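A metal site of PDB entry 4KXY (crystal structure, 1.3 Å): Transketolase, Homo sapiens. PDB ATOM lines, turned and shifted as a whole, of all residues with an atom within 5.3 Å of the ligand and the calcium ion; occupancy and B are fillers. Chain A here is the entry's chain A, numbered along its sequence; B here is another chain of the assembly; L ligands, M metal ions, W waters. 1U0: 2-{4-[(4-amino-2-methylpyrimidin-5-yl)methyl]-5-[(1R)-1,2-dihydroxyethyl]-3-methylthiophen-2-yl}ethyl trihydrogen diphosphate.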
ATOM      1  N   HIS A  37      19.984  18.482  -4.135  1.00  0.00           N
ATOM      2  CA  HIS A  37      18.801  17.943  -4.726  1.00  0.00           C
ATOM      3  C   HIS A  37      19.018  17.241  -6.062  1.00  0.00           C
ATOM      4  O   HIS A  37      18.460  17.580  -7.127  1.00  0.00           O
ATOM      5  CB  HIS A  37      17.796  19.113  -4.906  1.00  0.00           C
ATOM      6  CG  HIS A  37      17.467  19.777  -3.592  1.00  0.00           C
ATOM      7  ND1 HIS A  37      18.367  20.612  -2.962  1.00  0.00           N
ATOM      8  CD2 HIS A  37      16.364  19.751  -2.828  1.00  0.00           C
ATOM      9  CE1 HIS A  37      17.837  21.072  -1.833  1.00  0.00           C
ATOM     10  NE2 HIS A  37      16.612  20.547  -1.731  1.00  0.00           N
ATOM     11  N   SER A  40      15.903  16.338  -8.182  1.00  0.00           N
ATOM     12  CA  SER A  40      15.265  17.511  -8.803  1.00  0.00           C
ATOM     13  C   SER A  40      16.034  17.989 -10.035  1.00  0.00           C
ATOM     14  O   SER A  40      15.492  18.588 -10.951  1.00  0.00           O
ATOM     15  CB  SER A  40      15.195  18.657  -7.802  1.00  0.00           C
ATOM     16  OG  SER A  40      14.395  18.294  -6.667  1.00  0.00           O
ATOM     17  N   SER A  43      15.282  15.125 -13.189  1.00  0.00           N
ATOM     18  CA  SER A  43      14.067  15.188 -14.000  1.00  0.00           C
ATOM     19  C   SER A  43      14.192  16.232 -15.095  1.00  0.00           C
ATOM     20  O   SER A  43      13.460  16.142 -16.106  1.00  0.00           O
ATOM     21  CB  SER A  43      12.865  15.542 -13.142  1.00  0.00           C
ATOM     22  OG  SER A  43      13.143  16.767 -12.483  1.00  0.00           O
ATOM     23  N   LYS A  75      12.716  26.839 -10.230  1.00  0.00           N
ATOM     24  CA  LYS A  75      12.931  25.745  -9.263  1.00  0.00           C
ATOM     25  C   LYS A  75      14.438  25.772  -8.942  1.00  0.00           C
ATOM     26  O   LYS A  75      15.257  24.950  -9.343  1.00  0.00           O
ATOM     27  CB  LYS A  75      12.391  24.400  -9.804  1.00  0.00           C
ATOM     28  CG  LYS A  75      12.735  24.013 -11.212  1.00  0.00           C
ATOM     29  CD  LYS A  75      12.426  22.566 -11.568  1.00  0.00           C
ATOM     30  CE  LYS A  75      13.598  21.665 -11.183  1.00  0.00           C
ATOM     31  NZ  LYS A  75      13.176  20.245 -11.274  1.00  0.00           N
ATOM     32  N   HIS A  77      16.457  25.166  -6.509  1.00  0.00           N
ATOM     33  CA  HIS A  77      17.121  24.073  -5.819  1.00  0.00           C
ATOM     34  C   HIS A  77      17.739  23.105  -6.800  1.00  0.00           C
ATOM     35  O   HIS A  77      18.539  22.224  -6.424  1.00  0.00           O
ATOM     36  CB  HIS A  77      16.182  23.398  -4.798  1.00  0.00           C
ATOM     37  CG  HIS A  77      14.911  22.894  -5.392  1.00  0.00           C
ATOM     38  ND1 HIS A  77      13.887  23.709  -5.835  1.00  0.00           N
ATOM     39  CD2 HIS A  77      14.516  21.634  -5.662  1.00  0.00           C
ATOM     40  CE1 HIS A  77      12.930  22.964  -6.335  1.00  0.00           C
ATOM     41  NE2 HIS A  77      13.278  21.701  -6.226  1.00  0.00           N
ATOM     42  N   HIS A 110      21.353  27.734  -3.799  1.00  0.00           N
ATOM     43  CA  HIS A 110      20.352  28.215  -4.780  1.00  0.00           C
ATOM     44  C   HIS A 110      21.027  29.326  -5.578  1.00  0.00           C
ATOM     45  O   HIS A 110      22.029  29.898  -5.120  1.00  0.00           O
ATOM     46  CB  HIS A 110      19.059  28.663  -4.115  1.00  0.00           C
ATOM     47  CG  HIS A 110      18.350  27.611  -3.346  1.00  0.00           C
ATOM     48  ND1 HIS A 110      18.755  27.090  -2.113  1.00  0.00           N
ATOM     49  CD2 HIS A 110      17.202  26.939  -3.626  1.00  0.00           C
ATOM     50  CE1 HIS A 110      17.879  26.174  -1.732  1.00  0.00           C
ATOM     51  NE2 HIS A 110      16.906  26.055  -2.629  1.00  0.00           N
ATOM     52  N   GLY A 123      14.906  30.472  -5.215  1.00  0.00           N
ATOM     53  CA  GLY A 123      14.982  29.616  -4.049  1.00  0.00           C
ATOM     54  C   GLY A 123      13.701  29.750  -3.255  1.00  0.00           C
ATOM     55  O   GLY A 123      13.356  28.766  -2.627  1.00  0.00           O
ATOM     56  N   SER A 124      13.033  30.903  -3.309  1.00  0.00           N
ATOM     57  CA  SER A 124      11.672  30.974  -2.803  1.00  0.00           C
ATOM     58  C   SER A 124      10.789  30.628  -4.012  1.00  0.00           C
ATOM     59  O   SER A 124      10.760  31.398  -4.962  1.00  0.00           O
ATOM     60  CB  SER A 124      11.355  32.329  -2.224  1.00  0.00           C
ATOM     61  OG  SER A 124       9.987  32.280  -1.911  1.00  0.00           O
ATOM     62  N   LEU A 125      10.144  29.477  -3.949  1.00  0.00           N
ATOM     63  CA  LEU A 125       9.418  28.981  -5.098  1.00  0.00           C
ATOM     64  C   LEU A 125       8.279  29.856  -5.584  1.00  0.00           C
ATOM     65  O   LEU A 125       7.627  30.555  -4.802  1.00  0.00           O
ATOM     66  CB  LEU A 125       8.858  27.588  -4.783  1.00  0.00           C
ATOM     67  CG  LEU A 125       9.955  26.513  -4.701  1.00  0.00           C
ATOM     68  CD1 LEU A 125       9.460  25.308  -3.923  1.00  0.00           C
ATOM     69  CD2 LEU A 125      10.409  26.122  -6.098  1.00  0.00           C
ATOM     70  N   GLY A 154       8.989  23.893 -11.315  1.00  0.00           N
ATOM     71  CA  GLY A 154       8.576  22.575 -10.807  1.00  0.00           C
ATOM     72  C   GLY A 154       7.037  22.466 -10.805  1.00  0.00           C
ATOM     73  O   GLY A 154       6.344  23.448 -10.950  1.00  0.00           O
ATOM     74  N   ASP A 155       6.531  21.252 -10.590  1.00  0.00           N
ATOM     75  CA  ASP A 155       5.066  21.091 -10.549  1.00  0.00           C
ATOM     76  C   ASP A 155       4.524  21.412  -9.170  1.00  0.00           C
ATOM     77  O   ASP A 155       3.465  22.052  -9.050  1.00  0.00           O
ATOM     78  CB  ASP A 155       4.576  19.749 -11.072  1.00  0.00           C
ATOM     79  CG  ASP A 155       5.203  18.513 -10.483  1.00  0.00           C
ATOM     80  OD1 ASP A 155       6.102  18.556  -9.623  1.00  0.00           O
ATOM     81  OD2 ASP A 155       4.754  17.427 -10.925  1.00  0.00           O
ATOM     82  N   GLY A 156       5.208  21.059  -8.085  1.00  0.00           N
ATOM     83  CA  GLY A 156       4.810  21.497  -6.742  1.00  0.00           C
ATOM     84  C   GLY A 156       4.730  23.026  -6.671  1.00  0.00           C
ATOM     85  O   GLY A 156       3.817  23.612  -6.092  1.00  0.00           O
ATOM     86  N   GLU A 157       5.734  23.672  -7.250  1.00  0.00           N
ATOM     87  CA  GLU A 157       5.870  25.127  -7.345  1.00  0.00           C
ATOM     88  C   GLU A 157       4.617  25.794  -7.879  1.00  0.00           C
ATOM     89  O   GLU A 157       4.336  26.942  -7.532  1.00  0.00           O
ATOM     90  CB  GLU A 157       7.094  25.365  -8.247  1.00  0.00           C
ATOM     91  CG  GLU A 157       7.348  26.839  -8.489  1.00  0.00           C
ATOM     92  CD  GLU A 157       8.684  27.136  -9.120  1.00  0.00           C
ATOM     93  OE1 GLU A 157       9.261  26.311  -9.851  1.00  0.00           O
ATOM     94  OE2 GLU A 157       9.099  28.287  -8.835  1.00  0.00           O
ATOM     95  N   GLU A 160       1.877  27.728  -5.968  1.00  0.00           N
ATOM     96  CA  GLU A 160       1.991  29.112  -5.535  1.00  0.00           C
ATOM     97  C   GLU A 160       1.146  30.057  -6.403  1.00  0.00           C
ATOM     98  O   GLU A 160       1.242  30.087  -7.627  1.00  0.00           O
ATOM     99  CB  GLU A 160       3.411  29.621  -5.552  1.00  0.00           C
ATOM    100  CG  GLU A 160       4.306  29.007  -4.494  1.00  0.00           C
ATOM    101  CD  GLU A 160       4.114  29.569  -3.111  1.00  0.00           C
ATOM    102  OE1 GLU A 160       3.200  30.386  -2.875  1.00  0.00           O
ATOM    103  OE2 GLU A 160       4.920  29.152  -2.245  1.00  0.00           O
ATOM    104  N   ASP A 183       8.213  21.190 -15.272  1.00  0.00           N
ATOM    105  CA  ASP A 183       8.842  19.900 -14.992  1.00  0.00           C
ATOM    106  C   ASP A 183       7.858  19.052 -14.157  1.00  0.00           C
ATOM    107  O   ASP A 183       7.840  19.106 -12.930  1.00  0.00           O
ATOM    108  CB  ASP A 183      10.176  20.117 -14.266  1.00  0.00           C
ATOM    109  CG  ASP A 183      10.971  18.841 -13.972  1.00  0.00           C
ATOM    110  OD1 ASP A 183      10.467  17.748 -14.263  1.00  0.00           O
ATOM    111  OD2 ASP A 183      12.114  18.995 -13.473  1.00  0.00           O
ATOM    112  N   ASN A 185       7.215  16.213 -12.774  1.00  0.00           N
ATOM    113  CA  ASN A 185       7.807  14.971 -12.309  1.00  0.00           C
ATOM    114  C   ASN A 185       7.041  14.307 -11.151  1.00  0.00           C
ATOM    115  O   ASN A 185       7.592  13.387 -10.512  1.00  0.00           O
ATOM    116  CB  ASN A 185       9.273  15.224 -11.957  1.00  0.00           C
ATOM    117  CG  ASN A 185       9.431  16.015 -10.755  1.00  0.00           C
ATOM    118  OD1 ASN A 185       8.606  16.202  -9.892  1.00  0.00           O
ATOM    119  ND2 ASN A 185      10.577  16.522 -10.378  1.00  0.00           N
ATOM    120  N   ARG A 186       5.820  14.711 -10.932  1.00  0.00           N
ATOM    121  CA  ARG A 186       4.834  14.015 -10.084  1.00  0.00           C
ATOM    122  C   ARG A 186       4.941  14.240  -8.587  1.00  0.00           C
ATOM    123  O   ARG A 186       3.925  14.184  -7.876  1.00  0.00           O
ATOM    124  CB  ARG A 186       4.847  12.482 -10.368  1.00  0.00           C
ATOM    125  CG  ARG A 186       3.575  11.781  -9.996  1.00  0.00           C
ATOM    126  CD  ARG A 186       3.633  10.280 -10.292  1.00  0.00           C
ATOM    127  NE  ARG A 186       4.629   9.564  -9.524  1.00  0.00           N
ATOM    128  CZ  ARG A 186       4.504   9.150  -8.263  1.00  0.00           C
ATOM    129  NH1 ARG A 186       5.485   8.498  -7.678  1.00  0.00           N
ATOM    130  NH2 ARG A 186       3.384   9.417  -7.569  1.00  0.00           N
ATOM    131  N   LEU A 187       6.175  14.485  -8.114  1.00  0.00           N
ATOM    132  CA  LEU A 187       6.394  14.544  -6.694  1.00  0.00           C
ATOM    133  C   LEU A 187       6.857  15.911  -6.212  1.00  0.00           C
ATOM    134  O   LEU A 187       7.640  16.581  -6.863  1.00  0.00           O
ATOM    135  CB  LEU A 187       7.456  13.508  -6.312  1.00  0.00           C
ATOM    136  CG  LEU A 187       7.111  12.036  -6.655  1.00  0.00           C
ATOM    137  CD1 LEU A 187       8.267  11.138  -6.343  1.00  0.00           C
ATOM    138  CD2 LEU A 187       5.889  11.627  -5.820  1.00  0.00           C
ATOM    139  N   GLY A 188       6.401  16.319  -5.043  1.00  0.00           N
ATOM    140  CA  GLY A 188       6.920  17.498  -4.394  1.00  0.00           C
ATOM    141  C   GLY A 188       8.027  17.123  -3.416  1.00  0.00           C
ATOM    142  O   GLY A 188       8.788  16.167  -3.637  1.00  0.00           O
ATOM    143  N   GLN A 189       8.128  17.903  -2.346  1.00  0.00           N
ATOM    144  CA  GLN A 189       9.161  17.613  -1.346  1.00  0.00           C
ATOM    145  C   GLN A 189       8.796  16.463  -0.431  1.00  0.00           C
ATOM    146  O   GLN A 189       9.634  15.598  -0.144  1.00  0.00           O
ATOM    147  CB  GLN A 189       9.449  18.860  -0.488  1.00  0.00           C
ATOM    148  CG  GLN A 189      10.205  18.564   0.800  1.00  0.00           C
ATOM    149  CD  GLN A 189      10.837  19.757   1.474  1.00  0.00           C
ATOM    150  OE1 GLN A 189      11.300  20.703   0.831  1.00  0.00           O
ATOM    151  NE2 GLN A 189      10.937  19.710   2.782  1.00  0.00           N
ATOM    152  N   LYS A 244      10.962  12.126 -11.381  1.00  0.00           N
ATOM    153  CA  LYS A 244      11.906  12.674 -10.414  1.00  0.00           C
ATOM    154  C   LYS A 244      13.007  11.648 -10.270  1.00  0.00           C
ATOM    155  O   LYS A 244      12.740  10.445 -10.197  1.00  0.00           O
ATOM    156  CB  LYS A 244      11.191  12.957  -9.099  1.00  0.00           C
ATOM    157  CG  LYS A 244      11.907  13.996  -8.258  1.00  0.00           C
ATOM    158  CD  LYS A 244      11.033  14.641  -7.195  1.00  0.00           C
ATOM    159  CE  LYS A 244      11.749  15.680  -6.353  1.00  0.00           C
ATOM    160  NZ  LYS A 244      10.704  16.615  -5.817  1.00  0.00           N
ATOM    161  N   HIS A 258      13.515  13.639  -2.029  1.00  0.00           N
ATOM    162  CA  HIS A 258      13.714  15.045  -2.272  1.00  0.00           C
ATOM    163  C   HIS A 258      14.771  15.658  -1.370  1.00  0.00           C
ATOM    164  O   HIS A 258      14.669  15.532  -0.162  1.00  0.00           O
ATOM    165  CB  HIS A 258      12.394  15.809  -2.014  1.00  0.00           C
ATOM    166  CG  HIS A 258      12.577  17.269  -2.241  1.00  0.00           C
ATOM    167  ND1 HIS A 258      12.582  17.869  -3.418  1.00  0.00           N
ATOM    168  CD2 HIS A 258      12.843  18.304  -1.421  1.00  0.00           C
ATOM    169  CE1 HIS A 258      12.721  19.188  -3.412  1.00  0.00           C
ATOM    170  NE2 HIS A 258      12.911  19.457  -2.151  1.00  0.00           N
ATOM    171  N   ASP A 398       7.854  38.497   0.499  1.00  0.00           N
ATOM    172  CA  ASP A 398       8.858  37.481   0.056  1.00  0.00           C
ATOM    173  C   ASP A 398       9.493  37.896  -1.262  1.00  0.00           C
ATOM    174  O   ASP A 398      10.691  37.638  -1.493  1.00  0.00           O
ATOM    175  CB  ASP A 398       8.198  36.125   0.003  1.00  0.00           C
ATOM    176  CG  ASP A 398       9.106  34.934  -0.082  1.00  0.00           C
ATOM    177  OD1 ASP A 398      10.344  35.045   0.229  1.00  0.00           O
ATOM    178  OD2 ASP A 398       8.575  33.858  -0.462  1.00  0.00           O
ATOM    179  N   GLY B 340       3.032  23.419   4.630  1.00  0.00           N
ATOM    180  CA  GLY B 340       3.132  23.689   3.191  1.00  0.00           C
ATOM    181  C   GLY B 340       4.200  22.862   2.486  1.00  0.00           C
ATOM    182  O   GLY B 340       5.235  23.411   2.044  1.00  0.00           O
ATOM    183  N   ASP B 341       4.040  21.541   2.400  1.00  0.00           N
ATOM    184  CA  ASP B 341       4.961  20.611   1.765  1.00  0.00           C
ATOM    185  C   ASP B 341       6.345  20.676   2.392  1.00  0.00           C
ATOM    186  O   ASP B 341       7.288  20.349   1.693  1.00  0.00           O
ATOM    187  CB  ASP B 341       5.002  20.764   0.264  1.00  0.00           C
ATOM    188  CG  ASP B 341       5.702  19.664  -0.480  1.00  0.00           C
ATOM    189  OD1 ASP B 341       5.581  18.502   0.004  1.00  0.00           O
ATOM    190  OD2 ASP B 341       6.297  19.918  -1.557  1.00  0.00           O
ATOM    191  N   THR B 342       6.424  21.017   3.695  1.00  0.00           N
ATOM    192  CA  THR B 342       7.689  21.012   4.379  1.00  0.00           C
ATOM    193  C   THR B 342       7.666  20.141   5.622  1.00  0.00           C
ATOM    194  O   THR B 342       8.544  20.270   6.481  1.00  0.00           O
ATOM    195  CB  THR B 342       8.195  22.425   4.692  1.00  0.00           C
ATOM    196  OG1 THR B 342       7.227  23.168   5.426  1.00  0.00           O
ATOM    197  CG2 THR B 342       8.509  23.197   3.426  1.00  0.00           C
ATOM    198  N   ILE B 364       2.518  23.882  -1.557  1.00  0.00           N
ATOM    199  CA  ILE B 364       3.437  25.033  -1.572  1.00  0.00           C
ATOM    200  C   ILE B 364       2.646  26.302  -1.851  1.00  0.00           C
ATOM    201  O   ILE B 364       2.562  26.817  -2.968  1.00  0.00           O
ATOM    202  CB  ILE B 364       4.621  24.791  -2.532  1.00  0.00           C
ATOM    203  CG1 ILE B 364       5.294  23.447  -2.330  1.00  0.00           C
ATOM    204  CG2 ILE B 364       5.624  25.915  -2.380  1.00  0.00           C
ATOM    205  CD1 ILE B 364       6.313  23.066  -3.375  1.00  0.00           C
ATOM    206  N   GLU B 366       1.759  29.185   0.944  1.00  0.00           N
ATOM    207  CA  GLU B 366       1.786  29.708   2.301  1.00  0.00           C
ATOM    208  C   GLU B 366       0.702  30.720   2.594  1.00  0.00           C
ATOM    209  O   GLU B 366       0.172  30.762   3.722  1.00  0.00           O
ATOM    210  CB  GLU B 366       3.144  30.290   2.607  1.00  0.00           C
ATOM    211  CG  GLU B 366       4.298  29.301   2.540  1.00  0.00           C
ATOM    212  CD  GLU B 366       4.807  28.989   1.136  1.00  0.00           C
ATOM    213  OE1 GLU B 366       4.448  29.724   0.200  1.00  0.00           O
ATOM    214  OE2 GLU B 366       5.602  28.020   0.998  1.00  0.00           O
ATOM    215  N   THR B 388       6.035  26.011   8.331  1.00  0.00           N
ATOM    216  CA  THR B 388       6.880  26.038   7.164  1.00  0.00           C
ATOM    217  C   THR B 388       8.244  26.569   7.624  1.00  0.00           C
ATOM    218  O   THR B 388       8.458  26.762   8.849  1.00  0.00           O
ATOM    219  CB  THR B 388       6.274  26.874   6.027  1.00  0.00           C
ATOM    220  OG1 THR B 388       7.187  26.904   4.881  1.00  0.00           O
ATOM    221  CG2 THR B 388       6.033  28.306   6.381  1.00  0.00           C
ATOM    222  N   PHE B 389       9.134  26.850   6.673  1.00  0.00           N
ATOM    223  CA  PHE B 389      10.342  27.554   7.043  1.00  0.00           C
ATOM    224  C   PHE B 389       9.972  29.015   7.397  1.00  0.00           C
ATOM    225  O   PHE B 389       9.131  29.595   6.709  1.00  0.00           O
ATOM    226  CB  PHE B 389      11.329  27.604   5.903  1.00  0.00           C
ATOM    227  CG  PHE B 389      11.992  26.309   5.502  1.00  0.00           C
ATOM    228  CD1 PHE B 389      11.399  25.088   5.603  1.00  0.00           C
ATOM    229  CD2 PHE B 389      13.272  26.379   5.002  1.00  0.00           C
ATOM    230  CE1 PHE B 389      12.058  23.940   5.192  1.00  0.00           C
ATOM    231  CE2 PHE B 389      13.962  25.247   4.629  1.00  0.00           C
ATOM    232  CZ  PHE B 389      13.324  24.047   4.759  1.00  0.00           C
ATOM    233  N   PHE B 392       9.548  31.592   4.683  1.00  0.00           N
ATOM    234  CA  PHE B 392       8.396  31.591   3.789  1.00  0.00           C
ATOM    235  C   PHE B 392       7.144  32.088   4.491  1.00  0.00           C
ATOM    236  O   PHE B 392       6.152  32.297   3.777  1.00  0.00           O
ATOM    237  CB  PHE B 392       8.241  30.229   3.108  1.00  0.00           C
ATOM    238  CG  PHE B 392       9.534  29.733   2.460  1.00  0.00           C
ATOM    239  CD1 PHE B 392      10.216  30.628   1.621  1.00  0.00           C
ATOM    240  CD2 PHE B 392      10.061  28.474   2.706  1.00  0.00           C
ATOM    241  CE1 PHE B 392      11.413  30.286   1.060  1.00  0.00           C
ATOM    242  CE2 PHE B 392      11.284  28.147   2.119  1.00  0.00           C
ATOM    243  CZ  PHE B 392      11.940  29.059   1.354  1.00  0.00           C
ATOM    244  N   ARG B 395       5.999  35.266   2.780  1.00  0.00           N
ATOM    245  CA  ARG B 395       5.072  35.101   1.662  1.00  0.00           C
ATOM    246  C   ARG B 395       3.628  35.377   2.089  1.00  0.00           C
ATOM    247  O   ARG B 395       2.791  35.727   1.274  1.00  0.00           O
ATOM    248  CB  ARG B 395       5.181  33.691   1.095  1.00  0.00           C
ATOM    249  CG  ARG B 395       4.295  33.443  -0.120  1.00  0.00           C
ATOM    250  CD  ARG B 395       4.793  34.250  -1.328  1.00  0.00           C
ATOM    251  NE  ARG B 395       6.023  33.604  -1.794  1.00  0.00           N
ATOM    252  CZ  ARG B 395       6.224  32.969  -2.929  1.00  0.00           C
ATOM    253  NH1 ARG B 395       7.411  32.424  -3.157  1.00  0.00           N
ATOM    254  NH2 ARG B 395       5.384  32.811  -3.932  1.00  0.00           N
ATOM    255  N   ASP B 424      22.049  25.603   2.393  1.00  0.00           N
ATOM    256  CA  ASP B 424      21.008  25.995   1.442  1.00  0.00           C
ATOM    257  C   ASP B 424      21.154  27.436   1.006  1.00  0.00           C
ATOM    258  O   ASP B 424      20.700  27.826  -0.080  1.00  0.00           O
ATOM    259  CB  ASP B 424      19.638  25.745   2.052  1.00  0.00           C
ATOM    260  CG  ASP B 424      19.006  24.425   1.736  1.00  0.00           C
ATOM    261  OD1 ASP B 424      19.570  23.645   0.943  1.00  0.00           O
ATOM    262  OD2 ASP B 424      17.906  24.142   2.267  1.00  0.00           O
ATOM    263  N   GLN B 428      16.485  30.426   1.873  1.00  0.00           N
ATOM    264  CA  GLN B 428      15.844  29.608   2.868  1.00  0.00           C
ATOM    265  C   GLN B 428      16.019  30.142   4.310  1.00  0.00           C
ATOM    266  O   GLN B 428      15.449  29.540   5.198  1.00  0.00           O
ATOM    267  CB  GLN B 428      16.381  28.154   2.836  1.00  0.00           C
ATOM    268  CG  GLN B 428      16.477  27.543   1.454  1.00  0.00           C
ATOM    269  CD  GLN B 428      15.165  27.380   0.719  1.00  0.00           C
ATOM    270  OE1 GLN B 428      14.299  26.612   1.120  1.00  0.00           O
ATOM    271  NE2 GLN B 428      15.076  28.144  -0.392  1.00  0.00           N
HETATM  272  O3B 1U0 L   1      12.133  19.378  -6.955  1.00  0.00           O
HETATM  273  PB  1U0 L   1      11.033  19.386  -7.972  1.00  0.00           P
HETATM  274  O1B 1U0 L   1      10.149  18.168  -7.814  1.00  0.00           O
HETATM  275  O2B 1U0 L   1      11.421  19.604  -9.365  1.00  0.00           O
HETATM  276  O3A 1U0 L   1      10.092  20.722  -7.672  1.00  0.00           O
HETATM  277  PA  1U0 L   1       8.661  21.002  -7.009  1.00  0.00           P
HETATM  278  O1A 1U0 L   1       7.727  19.899  -7.469  1.00  0.00           O
HETATM  279  O2A 1U0 L   1       8.282  22.384  -7.270  1.00  0.00           O
HETATM  280  O7  1U0 L   1       8.848  20.724  -5.471  1.00  0.00           O
HETATM  281  C7  1U0 L   1       9.622  21.741  -4.751  1.00  0.00           C
HETATM  282  C6  1U0 L   1       9.647  21.226  -3.306  1.00  0.00           C
HETATM  283  C5  1U0 L   1      10.433  22.183  -2.445  1.00  0.00           C
HETATM  284  C4  1U0 L   1      10.058  22.908  -1.346  1.00  0.00           C
HETATM  285  CM4 1U0 L   1       8.664  22.805  -0.733  1.00  0.00           C
HETATM  286  S1  1U0 L   1      12.109  22.556  -2.835  1.00  0.00           S
HETATM  287  C2  1U0 L   1      12.246  23.640  -1.411  1.00  0.00           C
HETATM  288  C8  1U0 L   1      13.725  24.136  -1.116  1.00  0.00           C
HETATM  289  O9  1U0 L   1      14.175  25.197  -2.224  1.00  0.00           O
HETATM  290  C3  1U0 L   1      11.084  23.792  -0.778  1.00  0.00           C
HETATM  291  C7' 1U0 L   1      10.867  24.772   0.376  1.00  0.00           C
HETATM  292  C5' 1U0 L   1      10.093  25.902  -0.085  1.00  0.00           C
HETATM  293  C6' 1U0 L   1       8.797  26.189   0.441  1.00  0.00           C
HETATM  294  N1' 1U0 L   1       8.076  27.336   0.084  1.00  0.00           N
HETATM  295  C2' 1U0 L   1       8.633  28.221  -0.788  1.00  0.00           C
HETATM  296  CM2 1U0 L   1       7.884  29.518  -1.087  1.00  0.00           C
HETATM  297  N3' 1U0 L   1       9.829  28.039  -1.274  1.00  0.00           N
HETATM  298  C4' 1U0 L   1      10.565  26.946  -0.976  1.00  0.00           C
HETATM  299  N4' 1U0 L   1      11.818  26.827  -1.417  1.00  0.00           N
HETATM  300  C9  1U0 L   1      14.865  23.092  -1.317  1.00  0.00           C
HETATM  301  O10 1U0 L   1      14.386  21.805  -0.674  1.00  0.00           O
HETATM  302 CA    CA M   1       8.019  17.994  -8.605  1.00  0.00          CA
HETATM  303  O   HOH W   1      13.633  26.382  -4.759  1.00  0.00           O
HETATM  304  O   HOH W   2      15.294  24.107   1.848  1.00  0.00           O
HETATM  305  O   HOH W   3      13.448  21.885   1.872  1.00  0.00           O
HETATM  306  O   HOH W   4       6.149  25.882   2.641  1.00  0.00           O
HETATM  307  O   HOH W   5       8.936  19.262 -10.507  1.00  0.00           O
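OG of Ser 40 sits at hydrogen-bond distance from O3B of the ligand, at 2.5 Å. NZ of Lys 244 is in salt-bridge range of O3B of the ligand. NZ of Lys 75 is in salt-bridge range of O2B of the ligand (2.7 Å). NE2 of His 77 lies within hydrogen-bond range of O3B of the ligand (2.7 Å). The side-chain carboxylate of Glu 366 of chain B sits at hydrogen-bond distance from a nitrogen (N1') of the ligand, 2.7 Å away. O of Gly 123 is in hydrogen-bond range of N4' of the ligand (2.8 Å). NE2 of His 37 sits at hydrogen-bond distance from O10 of the ligand (2.8 Å). An oxygen (O2A) of the ligand sits at hydrogen-bond distance from the backbone NH of Gly 156 (3.4 Å). The backbone NH (N) of Glu 157 sits at hydrogen-bond distance from an oxygen (O2A) of the ligand (2.9 Å). A ring nitrogen (NE2) of His 110 sits at hydrogen-bond distance from an oxygen (O9) of the ligand (2.9 Å). N of Leu 125 sits at hydrogen-bond distance from N3' of the ligand (3.1 Å). A ring nitrogen (NE2) of His 258 lies within hydrogen-bond range of an oxygen (O10) of the ligand (3.1 Å).
OG of Ser 43 is in hydrogen-bond range of ND2 of Asn 185. The backbone carbonyl oxygen (O) of Ser 40 lies within hydrogen-bond range of the side-chain hydroxyl (OG) of Ser 43. The side-chain carboxylate of Glu 366 of chain B sits close to the side-chain carboxylate of Glu 160, 2.6 Å away. The side-chain carboxylate (OE1) of Glu 157 sits at hydrogen-bond distance from the backbone NH (N) of Gly 154 (2.8 Å). N of Glu 160 sits close to O of Ile 364 of chain B (3.2 Å). The side-chain carboxylate (OE1) of Glu 160 is in salt-bridge range of the guanidinium group (NH2) of Arg 395 of chain B, 3.4 Å away. OD2 of Asp 341 of chain B sits at hydrogen-bond distance from N of Gln 189 (2.8 Å). The side-chain hydroxyl (OG) of Ser 124 lies within hydrogen-bond range of the side-chain carboxylate (OD2) of Asp 398 (2.6 Å).
OG of Ser 124 touches CM2 of the ligand, at 3.6 Å. Gly 154 touches the ligand. OE2 of Glu 160 touches CM2 of the ligand, 3.2 Å away. CA of Gly 188 touches O7 of the ligand (3.9 Å). Gln 189 touches the ligand. Asp 341 of chain B touches the ligand (O to CM4, 3.7 Å). Ile 364 of chain B touches the ligand. CE2 of Phe 392 of chain B touches C5' of the ligand, 3.4 Å away. Arg 395 of chain B touches the ligand. Gln 428 of chain B touches the ligand (OE1 to C8, 3.4 Å). Of the 34 residues printed, 25 come within 4 Å of the ligand. Along chain A the residues within 4 Å of the ligand span positions 37 to 258. The nearest printed residue that does not touch the ligand is Thr 342 of chain B (4.2 Å).
The calcium ion is bound by O1A of the ligand, at 2.2 Å. OD1 of Asp 155 binds the calcium ion (2.2 Å). The backbone carbonyl oxygen (O) of Leu 187 binds the calcium ion (2.3 Å). An oxygen (O1B) of the ligand is bound to the calcium ion, 2.3 Å away. OD1 of Asn 185 binds the calcium ion (2.3 Å). Water W5 is bound to the calcium ion (2.5 Å). The calcium ion has six donor atoms within binding distance.
Water W5 lies within hydrogen-bond range of O of Asp 183 (2.7 Å), O2B of the ligand (2.8 Å), N of Asp 155 (3.1 Å) and ND2 of Asn 185 (3.2 Å). Water W3 lies within hydrogen-bond range of the side-chain amide oxygen (OE1) of Gln 189 (2.7 Å) and an oxygen (O10) of the ligand (2.7 Å). Water W1 lies within hydrogen-bond range of an oxygen (O9) of the ligand (2.9 Å), a ring nitrogen (ND1) of His 77 (2.9 Å) and the backbone carbonyl oxygen of Gly 123 (3.2 Å). Water W2 lies within hydrogen-bond range of OD2 of Asp 424 of chain B (2.6 Å) and OE1 of Gln 428 of chain B (2.8 Å). Water W4 lies within hydrogen-bond range of the side-chain hydroxyl (OG1) of Thr 388 of chain B, the backbone carbonyl oxygen (O) of Gly 340 of chain B and the side-chain carboxylate (OE2) of Glu 366 of chain B.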
